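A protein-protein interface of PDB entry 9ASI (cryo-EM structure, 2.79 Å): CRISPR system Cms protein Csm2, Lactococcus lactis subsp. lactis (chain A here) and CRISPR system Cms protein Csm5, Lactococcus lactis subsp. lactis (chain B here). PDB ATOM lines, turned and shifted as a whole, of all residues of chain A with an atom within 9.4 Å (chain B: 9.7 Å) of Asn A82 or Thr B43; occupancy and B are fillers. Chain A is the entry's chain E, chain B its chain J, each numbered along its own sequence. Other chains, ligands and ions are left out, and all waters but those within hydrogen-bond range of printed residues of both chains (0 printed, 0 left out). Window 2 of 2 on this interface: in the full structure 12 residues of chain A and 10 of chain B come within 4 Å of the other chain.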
ATOM      1  N   VAL A  67     -25.471  22.838 -21.069  1.00  0.00           N
ATOM      2  CA  VAL A  67     -24.552  21.716 -20.905  1.00  0.00           C
ATOM      3  C   VAL A  67     -24.949  20.571 -21.832  1.00  0.00           C
ATOM      4  O   VAL A  67     -24.098  19.959 -22.488  1.00  0.00           O
ATOM      5  CB  VAL A  67     -24.498  21.276 -19.432  1.00  0.00           C
ATOM      6  CG1 VAL A  67     -23.579  20.079 -19.270  1.00  0.00           C
ATOM      7  CG2 VAL A  67     -24.021  22.427 -18.573  1.00  0.00           C
ATOM      8  N   ARG A  70     -23.840  21.236 -25.388  1.00  0.00           N
ATOM      9  CA  ARG A  70     -22.433  20.915 -25.595  1.00  0.00           C
ATOM     10  C   ARG A  70     -22.161  19.416 -25.523  1.00  0.00           C
ATOM     11  O   ARG A  70     -21.164  18.954 -26.090  1.00  0.00           O
ATOM     12  CB  ARG A  70     -21.568  21.674 -24.590  1.00  0.00           C
ATOM     13  CG  ARG A  70     -21.611  23.177 -24.798  1.00  0.00           C
ATOM     14  CD  ARG A  70     -20.908  23.548 -26.099  1.00  0.00           C
ATOM     15  NE  ARG A  70     -20.838  24.990 -26.313  1.00  0.00           N
ATOM     16  CZ  ARG A  70     -21.729  25.692 -27.001  1.00  0.00           C
ATOM     17  NH1 ARG A  70     -22.774  25.114 -27.570  1.00  0.00           N
ATOM     18  NH2 ARG A  70     -21.564  27.005 -27.125  1.00  0.00           N
ATOM     19  N   VAL A  71     -23.024  18.649 -24.854  1.00  0.00           N
ATOM     20  CA  VAL A  71     -22.785  17.215 -24.706  1.00  0.00           C
ATOM     21  C   VAL A  71     -23.247  16.432 -25.934  1.00  0.00           C
ATOM     22  O   VAL A  71     -22.597  15.458 -26.333  1.00  0.00           O
ATOM     23  CB  VAL A  71     -23.453  16.699 -23.418  1.00  0.00           C
ATOM     24  CG1 VAL A  71     -23.413  15.183 -23.361  1.00  0.00           C
ATOM     25  CG2 VAL A  71     -22.737  17.261 -22.209  1.00  0.00           C
ATOM     26  N   THR A  74     -21.033  15.145 -28.996  1.00  0.00           N
ATOM     27  CA  THR A  74     -19.831  14.502 -28.465  1.00  0.00           C
ATOM     28  C   THR A  74     -20.148  13.021 -28.317  1.00  0.00           C
ATOM     29  O   THR A  74     -20.943  12.649 -27.449  1.00  0.00           O
ATOM     30  CB  THR A  74     -19.405  15.086 -27.113  1.00  0.00           C
ATOM     31  OG1 THR A  74     -20.408  14.803 -26.129  1.00  0.00           O
ATOM     32  CG2 THR A  74     -19.159  16.592 -27.177  1.00  0.00           C
ATOM     33  N   GLU A  78     -17.695   8.483 -21.742  1.00  0.00           N
ATOM     34  CA  GLU A  78     -17.476   9.225 -20.510  1.00  0.00           C
ATOM     35  C   GLU A  78     -17.410  10.715 -20.812  1.00  0.00           C
ATOM     36  O   GLU A  78     -16.941  11.122 -21.879  1.00  0.00           O
ATOM     37  CB  GLU A  78     -16.185   8.777 -19.819  1.00  0.00           C
ATOM     38  CG  GLU A  78     -14.968   8.777 -20.729  1.00  0.00           C
ATOM     39  CD  GLU A  78     -14.556   7.383 -21.156  1.00  0.00           C
ATOM     40  OE1 GLU A  78     -15.404   6.468 -21.108  1.00  0.00           O
ATOM     41  OE2 GLU A  78     -13.381   7.201 -21.541  1.00  0.00           O
ATOM     42  N   LEU A  79     -17.883  11.524 -19.867  1.00  0.00           N
ATOM     43  CA  LEU A  79     -17.861  12.971 -20.024  1.00  0.00           C
ATOM     44  C   LEU A  79     -16.482  13.526 -19.698  1.00  0.00           C
ATOM     45  O   LEU A  79     -15.812  13.064 -18.769  1.00  0.00           O
ATOM     46  CB  LEU A  79     -18.910  13.621 -19.123  1.00  0.00           C
ATOM     47  CG  LEU A  79     -20.355  13.182 -19.351  1.00  0.00           C
ATOM     48  CD1 LEU A  79     -21.257  13.780 -18.287  1.00  0.00           C
ATOM     49  CD2 LEU A  79     -20.814  13.583 -20.743  1.00  0.00           C
ATOM     50  N   SER A  80     -16.061  14.526 -20.467  1.00  0.00           N
ATOM     51  CA  SER A  80     -14.766  15.146 -20.249  1.00  0.00           C
ATOM     52  C   SER A  80     -14.791  16.009 -18.989  1.00  0.00           C
ATOM     53  O   SER A  80     -15.842  16.270 -18.397  1.00  0.00           O
ATOM     54  CB  SER A  80     -14.362  15.984 -21.462  1.00  0.00           C
ATOM     55  OG  SER A  80     -14.092  15.159 -22.581  1.00  0.00           O
ATOM     56  N   GLU A  81     -13.602  16.457 -18.579  1.00  0.00           N
ATOM     57  CA  GLU A  81     -13.492  17.273 -17.374  1.00  0.00           C
ATOM     58  C   GLU A  81     -14.208  18.608 -17.534  1.00  0.00           C
ATOM     59  O   GLU A  81     -14.696  19.172 -16.546  1.00  0.00           O
ATOM     60  CB  GLU A  81     -12.019  17.493 -17.025  1.00  0.00           C
ATOM     61  CG  GLU A  81     -11.283  16.229 -16.598  1.00  0.00           C
ATOM     62  CD  GLU A  81     -10.865  15.363 -17.774  1.00  0.00           C
ATOM     63  OE1 GLU A  81     -11.040  15.802 -18.930  1.00  0.00           O
ATOM     64  OE2 GLU A  81     -10.363  14.243 -17.542  1.00  0.00           O
ATOM     65  N   ASN A  82     -14.282  19.127 -18.761  1.00  0.00           N
ATOM     66  CA  ASN A  82     -15.040  20.351 -19.001  1.00  0.00           C
ATOM     67  C   ASN A  82     -16.517  20.151 -18.690  1.00  0.00           C
ATOM     68  O   ASN A  82     -17.151  21.011 -18.069  1.00  0.00           O
ATOM     69  CB  ASN A  82     -14.852  20.807 -20.448  1.00  0.00           C
ATOM     70  CG  ASN A  82     -13.528  21.507 -20.672  1.00  0.00           C
ATOM     71  OD1 ASN A  82     -12.617  21.417 -19.848  1.00  0.00           O
ATOM     72  ND2 ASN A  82     -13.413  22.212 -21.793  1.00  0.00           N
ATOM     73  N   ILE A  83     -17.081  19.015 -19.105  1.00  0.00           N
ATOM     74  CA  ILE A  83     -18.486  18.737 -18.826  1.00  0.00           C
ATOM     75  C   ILE A  83     -18.707  18.542 -17.331  1.00  0.00           C
ATOM     76  O   ILE A  83     -19.745  18.936 -16.786  1.00  0.00           O
ATOM     77  CB  ILE A  83     -18.956  17.516 -19.636  1.00  0.00           C
ATOM     78  CG1 ILE A  83     -18.706  17.740 -21.129  1.00  0.00           C
ATOM     79  CG2 ILE A  83     -20.425  17.235 -19.376  1.00  0.00           C
ATOM     80  CD1 ILE A  83     -19.309  19.017 -21.672  1.00  0.00           C
ATOM     81  N   LEU A  84     -17.740  17.933 -16.641  1.00  0.00           N
ATOM     82  CA  LEU A  84     -17.866  17.769 -15.197  1.00  0.00           C
ATOM     83  C   LEU A  84     -17.824  19.114 -14.481  1.00  0.00           C
ATOM     84  O   LEU A  84     -18.569  19.336 -13.521  1.00  0.00           O
ATOM     85  CB  LEU A  84     -16.773  16.840 -14.669  1.00  0.00           C
ATOM     86  CG  LEU A  84     -17.081  15.337 -14.640  1.00  0.00           C
ATOM     87  CD1 LEU A  84     -18.262  15.046 -13.723  1.00  0.00           C
ATOM     88  CD2 LEU A  84     -17.327  14.773 -16.031  1.00  0.00           C
ATOM     89  N   ALA A  85     -16.964  20.029 -14.934  1.00  0.00           N
ATOM     90  CA  ALA A  85     -16.968  21.373 -14.363  1.00  0.00           C
ATOM     91  C   ALA A  85     -18.256  22.116 -14.693  1.00  0.00           C
ATOM     92  O   ALA A  85     -18.735  22.916 -13.881  1.00  0.00           O
ATOM     93  CB  ALA A  85     -15.758  22.162 -14.855  1.00  0.00           C
ATOM     94  N   ASP A  86     -18.830  21.865 -15.871  1.00  0.00           N
ATOM     95  CA  ASP A  86     -20.130  22.440 -16.201  1.00  0.00           C
ATOM     96  C   ASP A  86     -21.215  21.930 -15.259  1.00  0.00           C
ATOM     97  O   ASP A  86     -22.076  22.696 -14.820  1.00  0.00           O
ATOM     98  CB  ASP A  86     -20.487  22.126 -17.653  1.00  0.00           C
ATOM     99  CG  ASP A  86     -19.686  22.947 -18.640  1.00  0.00           C
ATOM    100  OD1 ASP A  86     -19.001  23.894 -18.199  1.00  0.00           O
ATOM    101  OD2 ASP A  86     -19.738  22.649 -19.852  1.00  0.00           O
ATOM    102  N   ILE A  87     -21.187  20.636 -14.939  1.00  0.00           N
ATOM    103  CA  ILE A  87     -22.151  20.081 -13.991  1.00  0.00           C
ATOM    104  C   ILE A  87     -21.917  20.650 -12.595  1.00  0.00           C
ATOM    105  O   ILE A  87     -22.866  20.896 -11.837  1.00  0.00           O
ATOM    106  CB  ILE A  87     -22.082  18.543 -14.005  1.00  0.00           C
ATOM    107  CG1 ILE A  87     -22.510  18.005 -15.373  1.00  0.00           C
ATOM    108  CG2 ILE A  87     -22.952  17.951 -12.907  1.00  0.00           C
ATOM    109  CD1 ILE A  87     -22.809  16.521 -15.389  1.00  0.00           C
ATOM    110  N   ALA A  88     -20.653  20.875 -12.234  1.00  0.00           N
ATOM    111  CA  ALA A  88     -20.355  21.509 -10.953  1.00  0.00           C
ATOM    112  C   ALA A  88     -20.923  22.922 -10.892  1.00  0.00           C
ATOM    113  O   ALA A  88     -21.496  23.330  -9.874  1.00  0.00           O
ATOM    114  CB  ALA A  88     -18.846  21.526 -10.720  1.00  0.00           C
ATOM    115  N   TYR A  89     -20.775  23.684 -11.975  1.00  0.00           N
ATOM    116  CA  TYR A  89     -21.364  25.016 -12.022  1.00  0.00           C
ATOM    117  C   TYR A  89     -22.887  24.949 -12.014  1.00  0.00           C
ATOM    118  O   TYR A  89     -23.544  25.839 -11.459  1.00  0.00           O
ATOM    119  CB  TYR A  89     -20.862  25.769 -13.252  1.00  0.00           C
ATOM    120  CG  TYR A  89     -21.068  27.263 -13.172  1.00  0.00           C
ATOM    121  CD1 TYR A  89     -20.451  28.017 -12.185  1.00  0.00           C
ATOM    122  CD2 TYR A  89     -21.879  27.918 -14.087  1.00  0.00           C
ATOM    123  CE1 TYR A  89     -20.637  29.381 -12.110  1.00  0.00           C
ATOM    124  CE2 TYR A  89     -22.072  29.281 -14.021  1.00  0.00           C
ATOM    125  CZ  TYR A  89     -21.448  30.008 -13.030  1.00  0.00           C
ATOM    126  OH  TYR A  89     -21.641  31.369 -12.963  1.00  0.00           O
ATOM    127  N   ILE A  90     -23.461  23.905 -12.617  1.00  0.00           N
ATOM    128  CA  ILE A  90     -24.896  23.662 -12.499  1.00  0.00           C
ATOM    129  C   ILE A  90     -25.284  23.546 -11.033  1.00  0.00           C
ATOM    130  O   ILE A  90     -26.246  24.169 -10.573  1.00  0.00           O
ATOM    131  CB  ILE A  90     -25.296  22.394 -13.276  1.00  0.00           C
ATOM    132  CG1 ILE A  90     -25.509  22.692 -14.759  1.00  0.00           C
ATOM    133  CG2 ILE A  90     -26.547  21.761 -12.677  1.00  0.00           C
ATOM    134  CD1 ILE A  90     -25.675  21.440 -15.594  1.00  0.00           C
ATOM    135  N   MET A 121     -22.444  12.844 -11.265  1.00  0.00           N
ATOM    136  CA  MET A 121     -21.054  13.180 -10.984  1.00  0.00           C
ATOM    137  C   MET A 121     -20.262  11.954 -10.552  1.00  0.00           C
ATOM    138  O   MET A 121     -19.059  11.867 -10.816  1.00  0.00           O
ATOM    139  CB  MET A 121     -20.983  14.262  -9.907  1.00  0.00           C
ATOM    140  CG  MET A 121     -21.129  15.681 -10.434  1.00  0.00           C
ATOM    141  SD  MET A 121     -19.542  16.497 -10.686  1.00  0.00           S
ATOM    142  CE  MET A 121     -19.018  16.753  -8.993  1.00  0.00           C
ATOM    143  N   ILE B  40     -14.185  35.159 -17.038  1.00  0.00           N
ATOM    144  CA  ILE B  40     -13.339  33.975 -17.037  1.00  0.00           C
ATOM    145  C   ILE B  40     -13.518  33.214 -18.341  1.00  0.00           C
ATOM    146  O   ILE B  40     -14.539  33.320 -19.027  1.00  0.00           O
ATOM    147  CB  ILE B  40     -13.625  33.036 -15.847  1.00  0.00           C
ATOM    148  CG1 ILE B  40     -15.051  32.503 -15.924  1.00  0.00           C
ATOM    149  CG2 ILE B  40     -13.426  33.770 -14.532  1.00  0.00           C
ATOM    150  CD1 ILE B  40     -15.326  31.401 -14.933  1.00  0.00           C
ATOM    151  N   ASP B  41     -12.507  32.417 -18.680  1.00  0.00           N
ATOM    152  CA  ASP B  41     -12.613  31.430 -19.745  1.00  0.00           C
ATOM    153  C   ASP B  41     -13.160  30.133 -19.151  1.00  0.00           C
ATOM    154  O   ASP B  41     -13.644  30.099 -18.016  1.00  0.00           O
ATOM    155  CB  ASP B  41     -11.263  31.238 -20.430  1.00  0.00           C
ATOM    156  CG  ASP B  41     -10.129  31.025 -19.446  1.00  0.00           C
ATOM    157  OD1 ASP B  41     -10.279  30.202 -18.518  1.00  0.00           O
ATOM    158  OD2 ASP B  41      -9.080  31.686 -19.600  1.00  0.00           O
ATOM    159  N   HIS B  42     -13.099  29.041 -19.913  1.00  0.00           N
ATOM    160  CA  HIS B  42     -13.629  27.764 -19.456  1.00  0.00           C
ATOM    161  C   HIS B  42     -12.552  26.704 -19.257  1.00  0.00           C
ATOM    162  O   HIS B  42     -12.419  26.173 -18.155  1.00  0.00           O
ATOM    163  CB  HIS B  42     -14.692  27.255 -20.436  1.00  0.00           C
ATOM    164  CG  HIS B  42     -15.571  26.188 -19.866  1.00  0.00           C
ATOM    165  ND1 HIS B  42     -15.248  24.850 -19.924  1.00  0.00           N
ATOM    166  CD2 HIS B  42     -16.758  26.260 -19.218  1.00  0.00           C
ATOM    167  CE1 HIS B  42     -16.200  24.144 -19.340  1.00  0.00           C
ATOM    168  NE2 HIS B  42     -17.127  24.975 -18.904  1.00  0.00           N
ATOM    169  N   THR B  43     -11.771  26.387 -20.294  1.00  0.00           N
ATOM    170  CA  THR B  43     -10.899  25.214 -20.239  1.00  0.00           C
ATOM    171  C   THR B  43      -9.786  25.386 -19.212  1.00  0.00           C
ATOM    172  O   THR B  43      -9.488  24.464 -18.436  1.00  0.00           O
ATOM    173  CB  THR B  43     -10.314  24.935 -21.625  1.00  0.00           C
ATOM    174  OG1 THR B  43     -11.377  24.724 -22.562  1.00  0.00           O
ATOM    175  CG2 THR B  43      -9.426  23.698 -21.590  1.00  0.00           C
ATOM    176  N   LYS B  44      -9.147  26.558 -19.200  1.00  0.00           N
ATOM    177  CA  LYS B  44      -8.094  26.806 -18.222  1.00  0.00           C
ATOM    178  C   LYS B  44      -8.653  26.786 -16.806  1.00  0.00           C
ATOM    179  O   LYS B  44      -7.994  26.306 -15.880  1.00  0.00           O
ATOM    180  CB  LYS B  44      -7.400  28.134 -18.516  1.00  0.00           C
ATOM    181  CG  LYS B  44      -6.065  28.295 -17.805  1.00  0.00           C
ATOM    182  CD  LYS B  44      -4.987  27.444 -18.459  1.00  0.00           C
ATOM    183  CE  LYS B  44      -4.740  27.867 -19.898  1.00  0.00           C
ATOM    184  NZ  LYS B  44      -3.345  27.577 -20.328  1.00  0.00           N
ATOM    185  N   PHE B  45      -9.873  27.298 -16.622  1.00  0.00           N
ATOM    186  CA  PHE B  45     -10.513  27.233 -15.312  1.00  0.00           C
ATOM    187  C   PHE B  45     -10.780  25.791 -14.895  1.00  0.00           C
ATOM    188  O   PHE B  45     -10.602  25.433 -13.724  1.00  0.00           O
ATOM    189  CB  PHE B  45     -11.811  28.038 -15.324  1.00  0.00           C
ATOM    190  CG  PHE B  45     -12.475  28.134 -13.983  1.00  0.00           C
ATOM    191  CD1 PHE B  45     -11.923  28.905 -12.976  1.00  0.00           C
ATOM    192  CD2 PHE B  45     -13.655  27.458 -13.730  1.00  0.00           C
ATOM    193  CE1 PHE B  45     -12.535  28.998 -11.742  1.00  0.00           C
ATOM    194  CE2 PHE B  45     -14.270  27.546 -12.500  1.00  0.00           C
ATOM    195  CZ  PHE B  45     -13.709  28.317 -11.503  1.00  0.00           C
ATOM    196  N   THR B  46     -11.217  24.950 -15.838  1.00  0.00           N
ATOM    197  CA  THR B  46     -11.438  23.539 -15.534  1.00  0.00           C
ATOM    198  C   THR B  46     -10.146  22.868 -15.092  1.00  0.00           C
ATOM    199  O   THR B  46     -10.119  22.143 -14.092  1.00  0.00           O
ATOM    200  CB  THR B  46     -12.014  22.812 -16.751  1.00  0.00           C
ATOM    201  OG1 THR B  46     -11.091  22.901 -17.843  1.00  0.00           O
ATOM    202  CG2 THR B  46     -13.347  23.410 -17.164  1.00  0.00           C
ATOM    203  N   LYS B  47      -9.058  23.105 -15.829  1.00  0.00           N
ATOM    204  CA  LYS B  47      -7.778  22.507 -15.456  1.00  0.00           C
ATOM    205  C   LYS B  47      -7.289  23.040 -14.113  1.00  0.00           C
ATOM    206  O   LYS B  47      -6.738  22.289 -13.297  1.00  0.00           O
ATOM    207  CB  LYS B  47      -6.740  22.758 -16.549  1.00  0.00           C
ATOM    208  CG  LYS B  47      -5.628  21.722 -16.591  1.00  0.00           C
ATOM    209  CD  LYS B  47      -6.094  20.436 -17.257  1.00  0.00           C
ATOM    210  CE  LYS B  47      -6.544  20.682 -18.689  1.00  0.00           C
ATOM    211  NZ  LYS B  47      -7.284  19.516 -19.247  1.00  0.00           N
ATOM    212  N   TYR B  48      -7.487  24.338 -13.869  1.00  0.00           N
ATOM    213  CA  TYR B  48      -7.093  24.943 -12.601  1.00  0.00           C
ATOM    214  C   TYR B  48      -7.836  24.307 -11.434  1.00  0.00           C
ATOM    215  O   TYR B  48      -7.236  23.987 -10.401  1.00  0.00           O
ATOM    216  CB  TYR B  48      -7.354  26.448 -12.660  1.00  0.00           C
ATOM    217  CG  TYR B  48      -7.211  27.176 -11.345  1.00  0.00           C
ATOM    218  CD1 TYR B  48      -5.960  27.504 -10.843  1.00  0.00           C
ATOM    219  CD2 TYR B  48      -8.331  27.549 -10.613  1.00  0.00           C
ATOM    220  CE1 TYR B  48      -5.828  28.175  -9.645  1.00  0.00           C
ATOM    221  CE2 TYR B  48      -8.208  28.219  -9.414  1.00  0.00           C
ATOM    222  CZ  TYR B  48      -6.955  28.532  -8.936  1.00  0.00           C
ATOM    223  OH  TYR B  48      -6.829  29.201  -7.742  1.00  0.00           O
ATOM    224  N   LEU B  49      -9.147  24.114 -11.583  1.00  0.00           N
ATOM    225  CA  LEU B  49      -9.919  23.451 -10.536  1.00  0.00           C
ATOM    226  C   LEU B  49      -9.495  21.996 -10.377  1.00  0.00           C
ATOM    227  O   LEU B  49      -9.480  21.467  -9.258  1.00  0.00           O
ATOM    228  CB  LEU B  49     -11.412  23.547 -10.837  1.00  0.00           C
ATOM    229  CG  LEU B  49     -12.078  24.879 -10.494  1.00  0.00           C
ATOM    230  CD1 LEU B  49     -13.590  24.737 -10.538  1.00  0.00           C
ATOM    231  CD2 LEU B  49     -11.616  25.382  -9.132  1.00  0.00           C
ATOM    232  N   LEU B  50      -9.154  21.331 -11.484  1.00  0.00           N
ATOM    233  CA  LEU B  50      -8.691  19.950 -11.404  1.00  0.00           C
ATOM    234  C   LEU B  50      -7.396  19.850 -10.607  1.00  0.00           C
ATOM    235  O   LEU B  50      -7.194  18.893  -9.851  1.00  0.00           O
ATOM    236  CB  LEU B  50      -8.505  19.373 -12.808  1.00  0.00           C
ATOM    237  CG  LEU B  50      -8.028  17.922 -12.887  1.00  0.00           C
ATOM    238  CD1 LEU B  50      -8.924  17.014 -12.058  1.00  0.00           C
ATOM    239  CD2 LEU B  50      -7.969  17.451 -14.332  1.00  0.00           C
ATOM    240  N   GLU B  51      -6.505  20.830 -10.764  1.00  0.00           N
ATOM    241  CA  GLU B  51      -5.278  20.886  -9.979  1.00  0.00           C
ATOM    242  C   GLU B  51      -5.440  21.678  -8.682  1.00  0.00           C
ATOM    243  O   GLU B  51      -4.446  22.185  -8.150  1.00  0.00           O
ATOM    244  CB  GLU B  51      -4.138  21.476 -10.813  1.00  0.00           C
ATOM    245  CG  GLU B  51      -3.641  20.561 -11.918  1.00  0.00           C
ATOM    246  CD  GLU B  51      -2.463  21.147 -12.670  1.00  0.00           C
ATOM    247  OE1 GLU B  51      -2.115  22.318 -12.413  1.00  0.00           O
ATOM    248  OE2 GLU B  51      -1.881  20.434 -13.515  1.00  0.00           O
ATOM    249  N   LEU B  55     -14.565  20.123  -6.966  1.00  0.00           N
ATOM    250  CA  LEU B  55     -15.693  20.889  -7.489  1.00  0.00           C
ATOM    251  C   LEU B  55     -16.858  20.926  -6.506  1.00  0.00           C
ATOM    252  O   LEU B  55     -17.543  21.948  -6.391  1.00  0.00           O
ATOM    253  CB  LEU B  55     -16.134  20.304  -8.829  1.00  0.00           C
ATOM    254  CG  LEU B  55     -15.019  19.784  -9.742  1.00  0.00           C
ATOM    255  CD1 LEU B  55     -15.605  19.154 -10.995  1.00  0.00           C
ATOM    256  CD2 LEU B  55     -14.044  20.897 -10.102  1.00  0.00           C
ATOM    257  N   PRO B  82      -4.781  33.434 -15.561  1.00  0.00           N
ATOM    258  CA  PRO B  82      -5.202  32.258 -16.343  1.00  0.00           C
ATOM    259  C   PRO B  82      -6.709  32.139 -16.528  1.00  0.00           C
ATOM    260  O   PRO B  82      -7.143  31.363 -17.389  1.00  0.00           O
ATOM    261  CB  PRO B  82      -4.651  31.077 -15.531  1.00  0.00           C
ATOM    262  CG  PRO B  82      -3.516  31.651 -14.766  1.00  0.00           C
ATOM    263  CD  PRO B  82      -3.950  33.037 -14.409  1.00  0.00           C
ATOM    264  N   LEU B  83      -7.512  32.874 -15.766  1.00  0.00           N
ATOM    265  CA  LEU B  83      -8.966  32.792 -15.845  1.00  0.00           C
ATOM    266  C   LEU B  83      -9.574  34.137 -16.229  1.00  0.00           C
ATOM    267  O   LEU B  83     -10.604  34.554 -15.696  1.00  0.00           O
ATOM    268  CB  LEU B  83      -9.542  32.244 -14.537  1.00  0.00           C
ATOM    269  CG  LEU B  83      -9.217  32.865 -13.169  1.00  0.00           C
ATOM    270  CD1 LEU B  83     -10.099  34.043 -12.788  1.00  0.00           C
ATOM    271  CD2 LEU B  83      -9.284  31.788 -12.093  1.00  0.00           C
ATOM    272  N   VAL B  84      -8.954  34.832 -17.181  1.00  0.00           N
ATOM    273  CA  VAL B  84      -9.541  36.006 -17.815  1.00  0.00           C
ATOM    274  C   VAL B  84      -9.330  35.893 -19.318  1.00  0.00           C
ATOM    275  O   VAL B  84      -8.255  35.488 -19.776  1.00  0.00           O
ATOM    276  CB  VAL B  84      -8.952  37.330 -17.275  1.00  0.00           C
ATOM    277  CG1 VAL B  84      -9.286  37.506 -15.807  1.00  0.00           C
ATOM    278  CG2 VAL B  84      -7.447  37.395 -17.492  1.00  0.00           C
ATOM    279  N   LYS B  85     -10.364  36.224 -20.087  1.00  0.00           N
ATOM    280  CA  LYS B  85     -10.258  36.212 -21.542  1.00  0.00           C
ATOM    281  C   LYS B  85     -10.494  37.575 -22.172  1.00  0.00           C
ATOM    282  O   LYS B  85      -9.746  37.968 -23.070  1.00  0.00           O
ATOM    283  CB  LYS B  85     -11.231  35.187 -22.147  1.00  0.00           C
ATOM    284  CG  LYS B  85     -12.655  35.250 -21.622  1.00  0.00           C
ATOM    285  CD  LYS B  85     -13.543  34.290 -22.399  1.00  0.00           C
ATOM    286  CE  LYS B  85     -14.990  34.367 -21.954  1.00  0.00           C
ATOM    287  NZ  LYS B  85     -15.860  33.481 -22.772  1.00  0.00           N
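No residue of chain B comes within 4 Å of Ile A83. Of the printed residues of chain B, Leu A84 touches Leu B55. Of the printed residues of chain B, Ala A88 touches Leu B55. His B42 touches two residues of chain A. Printed residues of chain A within 4 Å of Thr B43: Asn A82. Thr B46 touches just these residues of chain A: Asn A82 (2.9 Å) and Ala A85 (3.6 Å). The nearest printed residue of chain A that does not touch Thr B43 is Glu A81 (7.5 Å).
The side-chain amide nitrogen (ND2) of Asn A82 sits at hydrogen-bond distance from the side-chain hydroxyl (OG1) of Thr B43, 3.3 Å away. The side-chain amide oxygen (OD1) of Asn A82 is in hydrogen-bond range of the side-chain hydroxyl (OG1) of Thr B46 (2.9 Å). NE2 of His B42 sits close to OD1 of Asp A86 (2.3 Å).
Hydrophobic or aromatic side chains of chain B that line the printed part of chain A: His B42 and Leu B55. Of the 18 printed residues of chain A, 5 touch a printed residue of chain B. Hydrophobic or aromatic side chains of chain A within 4 Å of the printed part of chain B: Ala A85 and Ala A88.
His B42 touches Asn A82. O of Leu A84 touches CD1 of Leu B55, at 3.9 Å. Ala A85 touches Thr B46. Ala A88 touches Leu B55 (CB to CB, 3.5 Å).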
